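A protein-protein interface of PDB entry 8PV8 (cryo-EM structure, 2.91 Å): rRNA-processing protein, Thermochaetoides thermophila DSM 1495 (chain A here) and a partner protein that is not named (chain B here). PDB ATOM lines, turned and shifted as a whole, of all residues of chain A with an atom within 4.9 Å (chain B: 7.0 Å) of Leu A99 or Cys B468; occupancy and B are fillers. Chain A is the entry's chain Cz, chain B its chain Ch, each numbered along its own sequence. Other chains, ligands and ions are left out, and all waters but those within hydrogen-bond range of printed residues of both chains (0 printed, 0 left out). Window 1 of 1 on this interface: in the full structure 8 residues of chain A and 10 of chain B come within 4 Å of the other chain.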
ATOM      1  N   ARG A  95      18.210 -14.590  20.609  1.00  0.00           N
ATOM      2  CA  ARG A  95      17.742 -13.498  21.462  1.00  0.00           C
ATOM      3  C   ARG A  95      17.083 -12.398  20.638  1.00  0.00           C
ATOM      4  O   ARG A  95      16.016 -11.882  21.007  1.00  0.00           O
ATOM      5  CB  ARG A  95      18.903 -12.931  22.280  1.00  0.00           C
ATOM      6  CG  ARG A  95      18.544 -11.690  23.084  1.00  0.00           C
ATOM      7  CD  ARG A  95      19.777 -11.032  23.679  1.00  0.00           C
ATOM      8  NE  ARG A  95      20.669 -10.510  22.651  1.00  0.00           N
ATOM      9  CZ  ARG A  95      21.782  -9.832  22.898  1.00  0.00           C
ATOM     10  NH1 ARG A  95      22.176  -9.580  24.136  1.00  0.00           N
ATOM     11  NH2 ARG A  95      22.518  -9.401  21.878  1.00  0.00           N
ATOM     12  N   TYR A  96      17.689 -12.052  19.502  1.00  0.00           N
ATOM     13  CA  TYR A  96      17.154 -11.057  18.589  1.00  0.00           C
ATOM     14  C   TYR A  96      15.841 -11.497  17.957  1.00  0.00           C
ATOM     15  O   TYR A  96      15.001 -10.642  17.657  1.00  0.00           O
ATOM     16  CB  TYR A  96      18.196 -10.770  17.506  1.00  0.00           C
ATOM     17  CG  TYR A  96      19.137  -9.632  17.838  1.00  0.00           C
ATOM     18  CD1 TYR A  96      19.455  -9.332  19.157  1.00  0.00           C
ATOM     19  CD2 TYR A  96      19.764  -8.906  16.834  1.00  0.00           C
ATOM     20  CE1 TYR A  96      20.327  -8.306  19.468  1.00  0.00           C
ATOM     21  CE2 TYR A  96      20.637  -7.877  17.135  1.00  0.00           C
ATOM     22  CZ  TYR A  96      20.917  -7.584  18.453  1.00  0.00           C
ATOM     23  OH  TYR A  96      21.790  -6.566  18.757  1.00  0.00           O
ATOM     24  N   GLU A  97      15.646 -12.800  17.748  1.00  0.00           N
ATOM     25  CA  GLU A  97      14.350 -13.290  17.286  1.00  0.00           C
ATOM     26  C   GLU A  97      13.275 -13.215  18.373  1.00  0.00           C
ATOM     27  O   GLU A  97      12.158 -12.738  18.117  1.00  0.00           O
ATOM     28  CB  GLU A  97      14.494 -14.728  16.774  1.00  0.00           C
ATOM     29  CG  GLU A  97      13.262 -15.284  16.075  1.00  0.00           C
ATOM     30  CD  GLU A  97      12.362 -16.070  17.009  1.00  0.00           C
ATOM     31  OE1 GLU A  97      12.880 -16.654  17.984  1.00  0.00           O
ATOM     32  OE2 GLU A  97      11.135 -16.102  16.771  1.00  0.00           O
ATOM     33  N   GLN A  98      13.597 -13.678  19.587  1.00  0.00           N
ATOM     34  CA  GLN A  98      12.590 -13.752  20.645  1.00  0.00           C
ATOM     35  C   GLN A  98      12.155 -12.370  21.114  1.00  0.00           C
ATOM     36  O   GLN A  98      10.987 -12.176  21.474  1.00  0.00           O
ATOM     37  CB  GLN A  98      13.101 -14.572  21.830  1.00  0.00           C
ATOM     38  CG  GLN A  98      13.453 -16.009  21.504  1.00  0.00           C
ATOM     39  CD  GLN A  98      13.393 -16.910  22.720  1.00  0.00           C
ATOM     40  OE1 GLN A  98      12.884 -16.520  23.770  1.00  0.00           O
ATOM     41  NE2 GLN A  98      13.922 -18.120  22.586  1.00  0.00           N
ATOM     42  N   LEU A  99      13.075 -11.398  21.128  1.00  0.00           N
ATOM     43  CA  LEU A  99      12.689 -10.044  21.517  1.00  0.00           C
ATOM     44  C   LEU A  99      11.688  -9.445  20.534  1.00  0.00           C
ATOM     45  O   LEU A  99      10.700  -8.819  20.944  1.00  0.00           O
ATOM     46  CB  LEU A  99      13.923  -9.153  21.623  1.00  0.00           C
ATOM     47  CG  LEU A  99      13.610  -7.734  22.091  1.00  0.00           C
ATOM     48  CD1 LEU A  99      13.022  -7.750  23.494  1.00  0.00           C
ATOM     49  CD2 LEU A  99      14.847  -6.880  22.032  1.00  0.00           C
ATOM     50  N   ALA A 100      11.921  -9.643  19.233  1.00  0.00           N
ATOM     51  CA  ALA A 100      10.993  -9.149  18.221  1.00  0.00           C
ATOM     52  C   ALA A 100       9.642  -9.844  18.324  1.00  0.00           C
ATOM     53  O   ALA A 100       8.595  -9.202  18.170  1.00  0.00           O
ATOM     54  CB  ALA A 100      11.588  -9.338  16.827  1.00  0.00           C
ATOM     55  N   ALA A 101       9.649 -11.155  18.593  1.00  0.00           N
ATOM     56  CA  ALA A 101       8.393 -11.882  18.770  1.00  0.00           C
ATOM     57  C   ALA A 101       7.610 -11.358  19.971  1.00  0.00           C
ATOM     58  O   ALA A 101       6.386 -11.177  19.901  1.00  0.00           O
ATOM     59  CB  ALA A 101       8.670 -13.378  18.918  1.00  0.00           C
ATOM     60  N   LYS A 102       8.309 -11.091  21.079  1.00  0.00           N
ATOM     61  CA  LYS A 102       7.659 -10.577  22.281  1.00  0.00           C
ATOM     62  C   LYS A 102       7.073  -9.186  22.048  1.00  0.00           C
ATOM     63  O   LYS A 102       5.952  -8.892  22.480  1.00  0.00           O
ATOM     64  CB  LYS A 102       8.659 -10.558  23.438  1.00  0.00           C
ATOM     65  CG  LYS A 102       8.169  -9.863  24.693  1.00  0.00           C
ATOM     66  CD  LYS A 102       9.254  -9.847  25.758  1.00  0.00           C
ATOM     67  CE  LYS A 102       8.825  -9.046  26.974  1.00  0.00           C
ATOM     68  NZ  LYS A 102       9.895  -8.993  28.007  1.00  0.00           N
ATOM     69  N   MET A 103       7.818  -8.318  21.355  1.00  0.00           N
ATOM     70  CA  MET A 103       7.317  -6.974  21.078  1.00  0.00           C
ATOM     71  C   MET A 103       6.118  -7.006  20.134  1.00  0.00           C
ATOM     72  O   MET A 103       5.164  -6.231  20.302  1.00  0.00           O
ATOM     73  CB  MET A 103       8.432  -6.102  20.503  1.00  0.00           C
ATOM     74  CG  MET A 103       9.542  -5.799  21.493  1.00  0.00           C
ATOM     75  SD  MET A 103       8.924  -4.988  22.978  1.00  0.00           S
ATOM     76  CE  MET A 103       9.406  -6.167  24.234  1.00  0.00           C
ATOM     77  N   HIS B 445       3.983   3.447  23.624  1.00  0.00           N
ATOM     78  CA  HIS B 445       4.979   2.425  23.883  1.00  0.00           C
ATOM     79  C   HIS B 445       4.356   1.247  24.632  1.00  0.00           C
ATOM     80  O   HIS B 445       3.326   1.366  25.296  1.00  0.00           O
ATOM     81  CB  HIS B 445       6.138   3.012  24.685  1.00  0.00           C
ATOM     82  CG  HIS B 445       7.024   3.922  23.890  1.00  0.00           C
ATOM     83  ND1 HIS B 445       7.780   3.483  22.825  1.00  0.00           N
ATOM     84  CD2 HIS B 445       7.268   5.248  24.004  1.00  0.00           C
ATOM     85  CE1 HIS B 445       8.455   4.500  22.320  1.00  0.00           C
ATOM     86  NE2 HIS B 445       8.162   5.583  23.017  1.00  0.00           N
ATOM     87  N   ALA B 447       6.772  -0.974  26.297  1.00  0.00           N
ATOM     88  CA  ALA B 447       7.809  -1.273  27.274  1.00  0.00           C
ATOM     89  C   ALA B 447       8.205   0.050  27.919  1.00  0.00           C
ATOM     90  O   ALA B 447       7.907   1.106  27.347  1.00  0.00           O
ATOM     91  CB  ALA B 447       8.995  -1.970  26.605  1.00  0.00           C
ATOM     92  N   GLY B 464      12.741   7.609  23.531  1.00  0.00           N
ATOM     93  CA  GLY B 464      13.351   6.328  23.249  1.00  0.00           C
ATOM     94  C   GLY B 464      13.033   5.338  24.343  1.00  0.00           C
ATOM     95  O   GLY B 464      13.296   5.614  25.525  1.00  0.00           O
ATOM     96  N   SER B 465      12.467   4.191  23.970  1.00  0.00           N
ATOM     97  CA  SER B 465      11.945   3.270  24.968  1.00  0.00           C
ATOM     98  C   SER B 465      12.583   1.892  24.845  1.00  0.00           C
ATOM     99  O   SER B 465      13.334   1.601  23.911  1.00  0.00           O
ATOM    100  CB  SER B 465      10.422   3.150  24.861  1.00  0.00           C
ATOM    101  OG  SER B 465       9.929   2.152  25.737  1.00  0.00           O
ATOM    102  N   LYS B 466      12.259   1.044  25.822  1.00  0.00           N
ATOM    103  CA  LYS B 466      12.755  -0.323  25.907  1.00  0.00           C
ATOM    104  C   LYS B 466      12.188  -1.220  24.809  1.00  0.00           C
ATOM    105  O   LYS B 466      12.792  -2.251  24.493  1.00  0.00           O
ATOM    106  CB  LYS B 466      12.430  -0.876  27.305  1.00  0.00           C
ATOM    107  CG  LYS B 466      12.880  -2.297  27.616  1.00  0.00           C
ATOM    108  CD  LYS B 466      12.403  -2.729  28.990  1.00  0.00           C
ATOM    109  CE  LYS B 466      12.858  -4.139  29.320  1.00  0.00           C
ATOM    110  NZ  LYS B 466      12.283  -4.610  30.609  1.00  0.00           N
ATOM    111  N   ASP B 467      11.093  -0.818  24.165  1.00  0.00           N
ATOM    112  CA  ASP B 467      10.471  -1.616  23.114  1.00  0.00           C
ATOM    113  C   ASP B 467      11.135  -1.440  21.752  1.00  0.00           C
ATOM    114  O   ASP B 467      10.469  -1.657  20.734  1.00  0.00           O
ATOM    115  CB  ASP B 467       8.972  -1.299  23.015  1.00  0.00           C
ATOM    116  CG  ASP B 467       8.684   0.168  22.721  1.00  0.00           C
ATOM    117  OD1 ASP B 467       9.625   0.978  22.614  1.00  0.00           O
ATOM    118  OD2 ASP B 467       7.491   0.512  22.595  1.00  0.00           O
ATOM    119  N   CYS B 468      12.398  -1.014  21.725  1.00  0.00           N
ATOM    120  CA  CYS B 468      13.287  -0.876  20.574  1.00  0.00           C
ATOM    121  C   CYS B 468      12.866   0.254  19.644  1.00  0.00           C
ATOM    122  O   CYS B 468      13.308   0.269  18.489  1.00  0.00           O
ATOM    123  CB  CYS B 468      13.405  -2.168  19.745  1.00  0.00           C
ATOM    124  SG  CYS B 468      13.588  -3.678  20.717  1.00  0.00           S
ATOM    125  N   THR B 469      12.036   1.195  20.089  1.00  0.00           N
ATOM    126  CA  THR B 469      11.514   2.232  19.214  1.00  0.00           C
ATOM    127  C   THR B 469      11.789   3.627  19.764  1.00  0.00           C
ATOM    128  O   THR B 469      11.853   3.857  20.985  1.00  0.00           O
ATOM    129  CB  THR B 469       9.999   2.080  18.987  1.00  0.00           C
ATOM    130  OG1 THR B 469       9.296   2.412  20.189  1.00  0.00           O
ATOM    131  CG2 THR B 469       9.631   0.668  18.550  1.00  0.00           C
ATOM    132  N   LEU B 470      11.945   4.561  18.821  1.00  0.00           N
ATOM    133  CA  LEU B 470      11.878   5.989  19.080  1.00  0.00           C
ATOM    134  C   LEU B 470      10.524   6.484  18.594  1.00  0.00           C
ATOM    135  O   LEU B 470      10.000   5.992  17.592  1.00  0.00           O
ATOM    136  CB  LEU B 470      12.979   6.760  18.347  1.00  0.00           C
ATOM    137  CG  LEU B 470      14.456   6.411  18.509  1.00  0.00           C
ATOM    138  CD1 LEU B 470      15.300   7.533  17.932  1.00  0.00           C
ATOM    139  CD2 LEU B 470      14.823   6.147  19.945  1.00  0.00           C
ATOM    140  N   LEU B 484       9.832   5.817  14.733  1.00  0.00           N
ATOM    141  CA  LEU B 484      11.174   5.477  14.275  1.00  0.00           C
ATOM    142  C   LEU B 484      11.519   4.083  14.788  1.00  0.00           C
ATOM    143  O   LEU B 484      11.997   3.921  15.925  1.00  0.00           O
ATOM    144  CB  LEU B 484      12.199   6.508  14.743  1.00  0.00           C
ATOM    145  CG  LEU B 484      11.934   7.954  14.318  1.00  0.00           C
ATOM    146  CD1 LEU B 484      12.989   8.879  14.906  1.00  0.00           C
ATOM    147  CD2 LEU B 484      11.859   8.092  12.803  1.00  0.00           C
ATOM    148  N   PRO B 485      11.239   3.051  13.998  1.00  0.00           N
ATOM    149  CA  PRO B 485      11.803   1.732  14.282  1.00  0.00           C
ATOM    150  C   PRO B 485      13.144   1.574  13.587  1.00  0.00           C
ATOM    151  O   PRO B 485      13.585   2.441  12.829  1.00  0.00           O
ATOM    152  CB  PRO B 485      10.760   0.773  13.704  1.00  0.00           C
ATOM    153  CG  PRO B 485      10.201   1.531  12.543  1.00  0.00           C
ATOM    154  CD  PRO B 485      10.226   2.996  12.929  1.00  0.00           C
ATOM    155  N   GLY B 486      13.791   0.444  13.845  1.00  0.00           N
ATOM    156  CA  GLY B 486      15.090   0.185  13.260  1.00  0.00           C
ATOM    157  C   GLY B 486      16.055  -0.402  14.265  1.00  0.00           C
ATOM    158  O   GLY B 486      16.905  -1.222  13.911  1.00  0.00           O
ATOM    159  N   HIS B 487      15.933   0.012  15.524  1.00  0.00           N
ATOM    160  CA  HIS B 487      16.660  -0.656  16.591  1.00  0.00           C
ATOM    161  C   HIS B 487      16.086  -2.048  16.799  1.00  0.00           C
ATOM    162  O   HIS B 487      14.868  -2.236  16.827  1.00  0.00           O
ATOM    163  CB  HIS B 487      16.579   0.151  17.887  1.00  0.00           C
ATOM    164  CG  HIS B 487      17.270   1.477  17.822  1.00  0.00           C
ATOM    165  ND1 HIS B 487      18.447   1.732  18.492  1.00  0.00           N
ATOM    166  CD2 HIS B 487      16.945   2.624  17.181  1.00  0.00           C
ATOM    167  CE1 HIS B 487      18.823   2.976  18.258  1.00  0.00           C
ATOM    168  NE2 HIS B 487      17.929   3.539  17.465  1.00  0.00           N
ATOM    169  N   GLU B 488      16.971  -3.034  16.920  1.00  0.00           N
ATOM    170  CA  GLU B 488      16.547  -4.411  17.112  1.00  0.00           C
ATOM    171  C   GLU B 488      16.551  -4.806  18.585  1.00  0.00           C
ATOM    172  O   GLU B 488      15.908  -5.795  18.957  1.00  0.00           O
ATOM    173  CB  GLU B 488      17.454  -5.343  16.287  1.00  0.00           C
ATOM    174  CG  GLU B 488      17.042  -6.809  16.229  1.00  0.00           C
ATOM    175  CD  GLU B 488      15.735  -7.026  15.488  1.00  0.00           C
ATOM    176  OE1 GLU B 488      15.399  -6.201  14.612  1.00  0.00           O
ATOM    177  OE2 GLU B 488      15.040  -8.022  15.781  1.00  0.00           O
ATOM    178  N   ASP B 489      17.196  -4.016  19.438  1.00  0.00           N
ATOM    179  CA  ASP B 489      17.261  -4.276  20.869  1.00  0.00           C
ATOM    180  C   ASP B 489      16.873  -2.990  21.594  1.00  0.00           C
ATOM    181  O   ASP B 489      16.442  -2.015  20.970  1.00  0.00           O
ATOM    182  CB  ASP B 489      18.652  -4.796  21.251  1.00  0.00           C
ATOM    183  CG  ASP B 489      18.616  -5.766  22.419  1.00  0.00           C
ATOM    184  OD1 ASP B 489      17.639  -5.736  23.193  1.00  0.00           O
ATOM    185  OD2 ASP B 489      19.568  -6.561  22.560  1.00  0.00           O
ATOM    186  N   GLU B 490      17.020  -2.994  22.919  1.00  0.00           N
ATOM    187  CA  GLU B 490      16.547  -1.886  23.740  1.00  0.00           C
ATOM    188  C   GLU B 490      17.330  -0.611  23.451  1.00  0.00           C
ATOM    189  O   GLU B 490      18.508  -0.656  23.092  1.00  0.00           O
ATOM    190  CB  GLU B 490      16.662  -2.239  25.223  1.00  0.00           C
ATOM    191  CG  GLU B 490      16.051  -3.576  25.600  1.00  0.00           C
ATOM    192  CD  GLU B 490      16.189  -3.881  27.079  1.00  0.00           C
ATOM    193  OE1 GLU B 490      16.456  -2.941  27.857  1.00  0.00           O
ATOM    194  OE2 GLU B 490      16.033  -5.059  27.463  1.00  0.00           O
ATOM    195  N   VAL B 491      16.659   0.527  23.599  1.00  0.00           N
ATOM    196  CA  VAL B 491      17.263   1.831  23.356  1.00  0.00           C
ATOM    197  C   VAL B 491      17.645   2.450  24.692  1.00  0.00           C
ATOM    198  O   VAL B 491      16.805   2.579  25.591  1.00  0.00           O
ATOM    199  CB  VAL B 491      16.302   2.744  22.578  1.00  0.00           C
ATOM    200  CG1 VAL B 491      16.921   4.109  22.376  1.00  0.00           C
ATOM    201  CG2 VAL B 491      15.945   2.119  21.242  1.00  0.00           C
ATOM    202  N   LYS B 508      21.191  -1.357  22.984  1.00  0.00           N
ATOM    203  CA  LYS B 508      21.771  -2.683  23.143  1.00  0.00           C
ATOM    204  C   LYS B 508      22.117  -3.338  21.812  1.00  0.00           C
ATOM    205  O   LYS B 508      22.720  -4.416  21.805  1.00  0.00           O
ATOM    206  CB  LYS B 508      20.814  -3.571  23.940  1.00  0.00           C
ATOM    207  CG  LYS B 508      21.488  -4.604  24.826  1.00  0.00           C
ATOM    208  CD  LYS B 508      20.477  -5.303  25.719  1.00  0.00           C
ATOM    209  CE  LYS B 508      21.110  -6.462  26.470  1.00  0.00           C
ATOM    210  NZ  LYS B 508      20.105  -7.233  27.251  1.00  0.00           N
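Arg A95 touches Asp B489.
Tyr A96 touches Asp B489.
O of Lys B508 touches OH of Tyr A96, at 3.8 Å.
Leu A99 touches Cys B468.
Glu B488 touches Leu A99.
Leu A99 touches Asp B489 (CD2 to OD1, 3.2 Å).
OE2 of Glu B488 touches CB of Ala A100, 3.8 Å away.
Met A103 touches Asp B467 (SD to CB, 3.7 Å).
The side-chain carboxylate of Glu B488 sits close to the backbone carbonyl oxygen of Tyr A96 (3.2 Å).
Of chain A, only Leu A99 comes within 4 Å of Cys B468.
Of the printed residues of chain A, Lys B508 touches Tyr A96.
Of the printed residues of chain A, Asp B467 touches Met A103.
Of the printed residues of chain B, Arg A95 touches Asp B489 (3.96 Å).
Of the printed residues of chain A, Asp B489 touches Arg A95, Tyr A96 and Leu A99.
His B445 touches none of the printed residues of chain A.
The nearest residue of chain B that does not touch Leu A99 is Glu B490 (4.5 Å).
The nearest residue of chain A that does not touch Cys B468 is Met A103 (4.6 Å).
The nearest printed residue of chain A that does not touch Asp B489 is Ala A100 (7.7 Å).
Of the 9 printed residues of chain A, 5 touch a printed residue of chain B.
Hydrophobic or aromatic side chains of chain A within 4 Å of the printed part of chain B: Tyr A96, Leu A99, Ala A100 and Met A103.
Printed residues of chain B that touch a printed residue of chain A: Asp B467, Cys B468, Glu B488, Asp B489 and Lys B508.
Along chain B the printed residues that touch a printed residue of chain A span positions 467 to 508.
Among the printed residues, 9 pairs touch across the chains.
The backbone carbonyl oxygen (O) of Asp B489 sits close to the side-chain sulfur (SG) of Cys B468 (3.3 Å).
OD1 of Asp B467 lies within hydrogen-bond range of OG1 of Thr B469, at 2.8 Å.
The side-chain carboxylate (OD2) of Asp B467 is in hydrogen-bond range of a ring nitrogen (ND1) of His B445.
N of Lys B508 sits at hydrogen-bond distance from O of Glu B490 (2.8 Å).
The side-chain sulfur of Cys B468 is in hydrogen-bond range of the backbone carbonyl oxygen of Glu B488, 3.6 Å away.
The side-chain carboxylate (OD1) of Asp B467 lies close to the side-chain hydroxyl (OG) of Ser B465.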
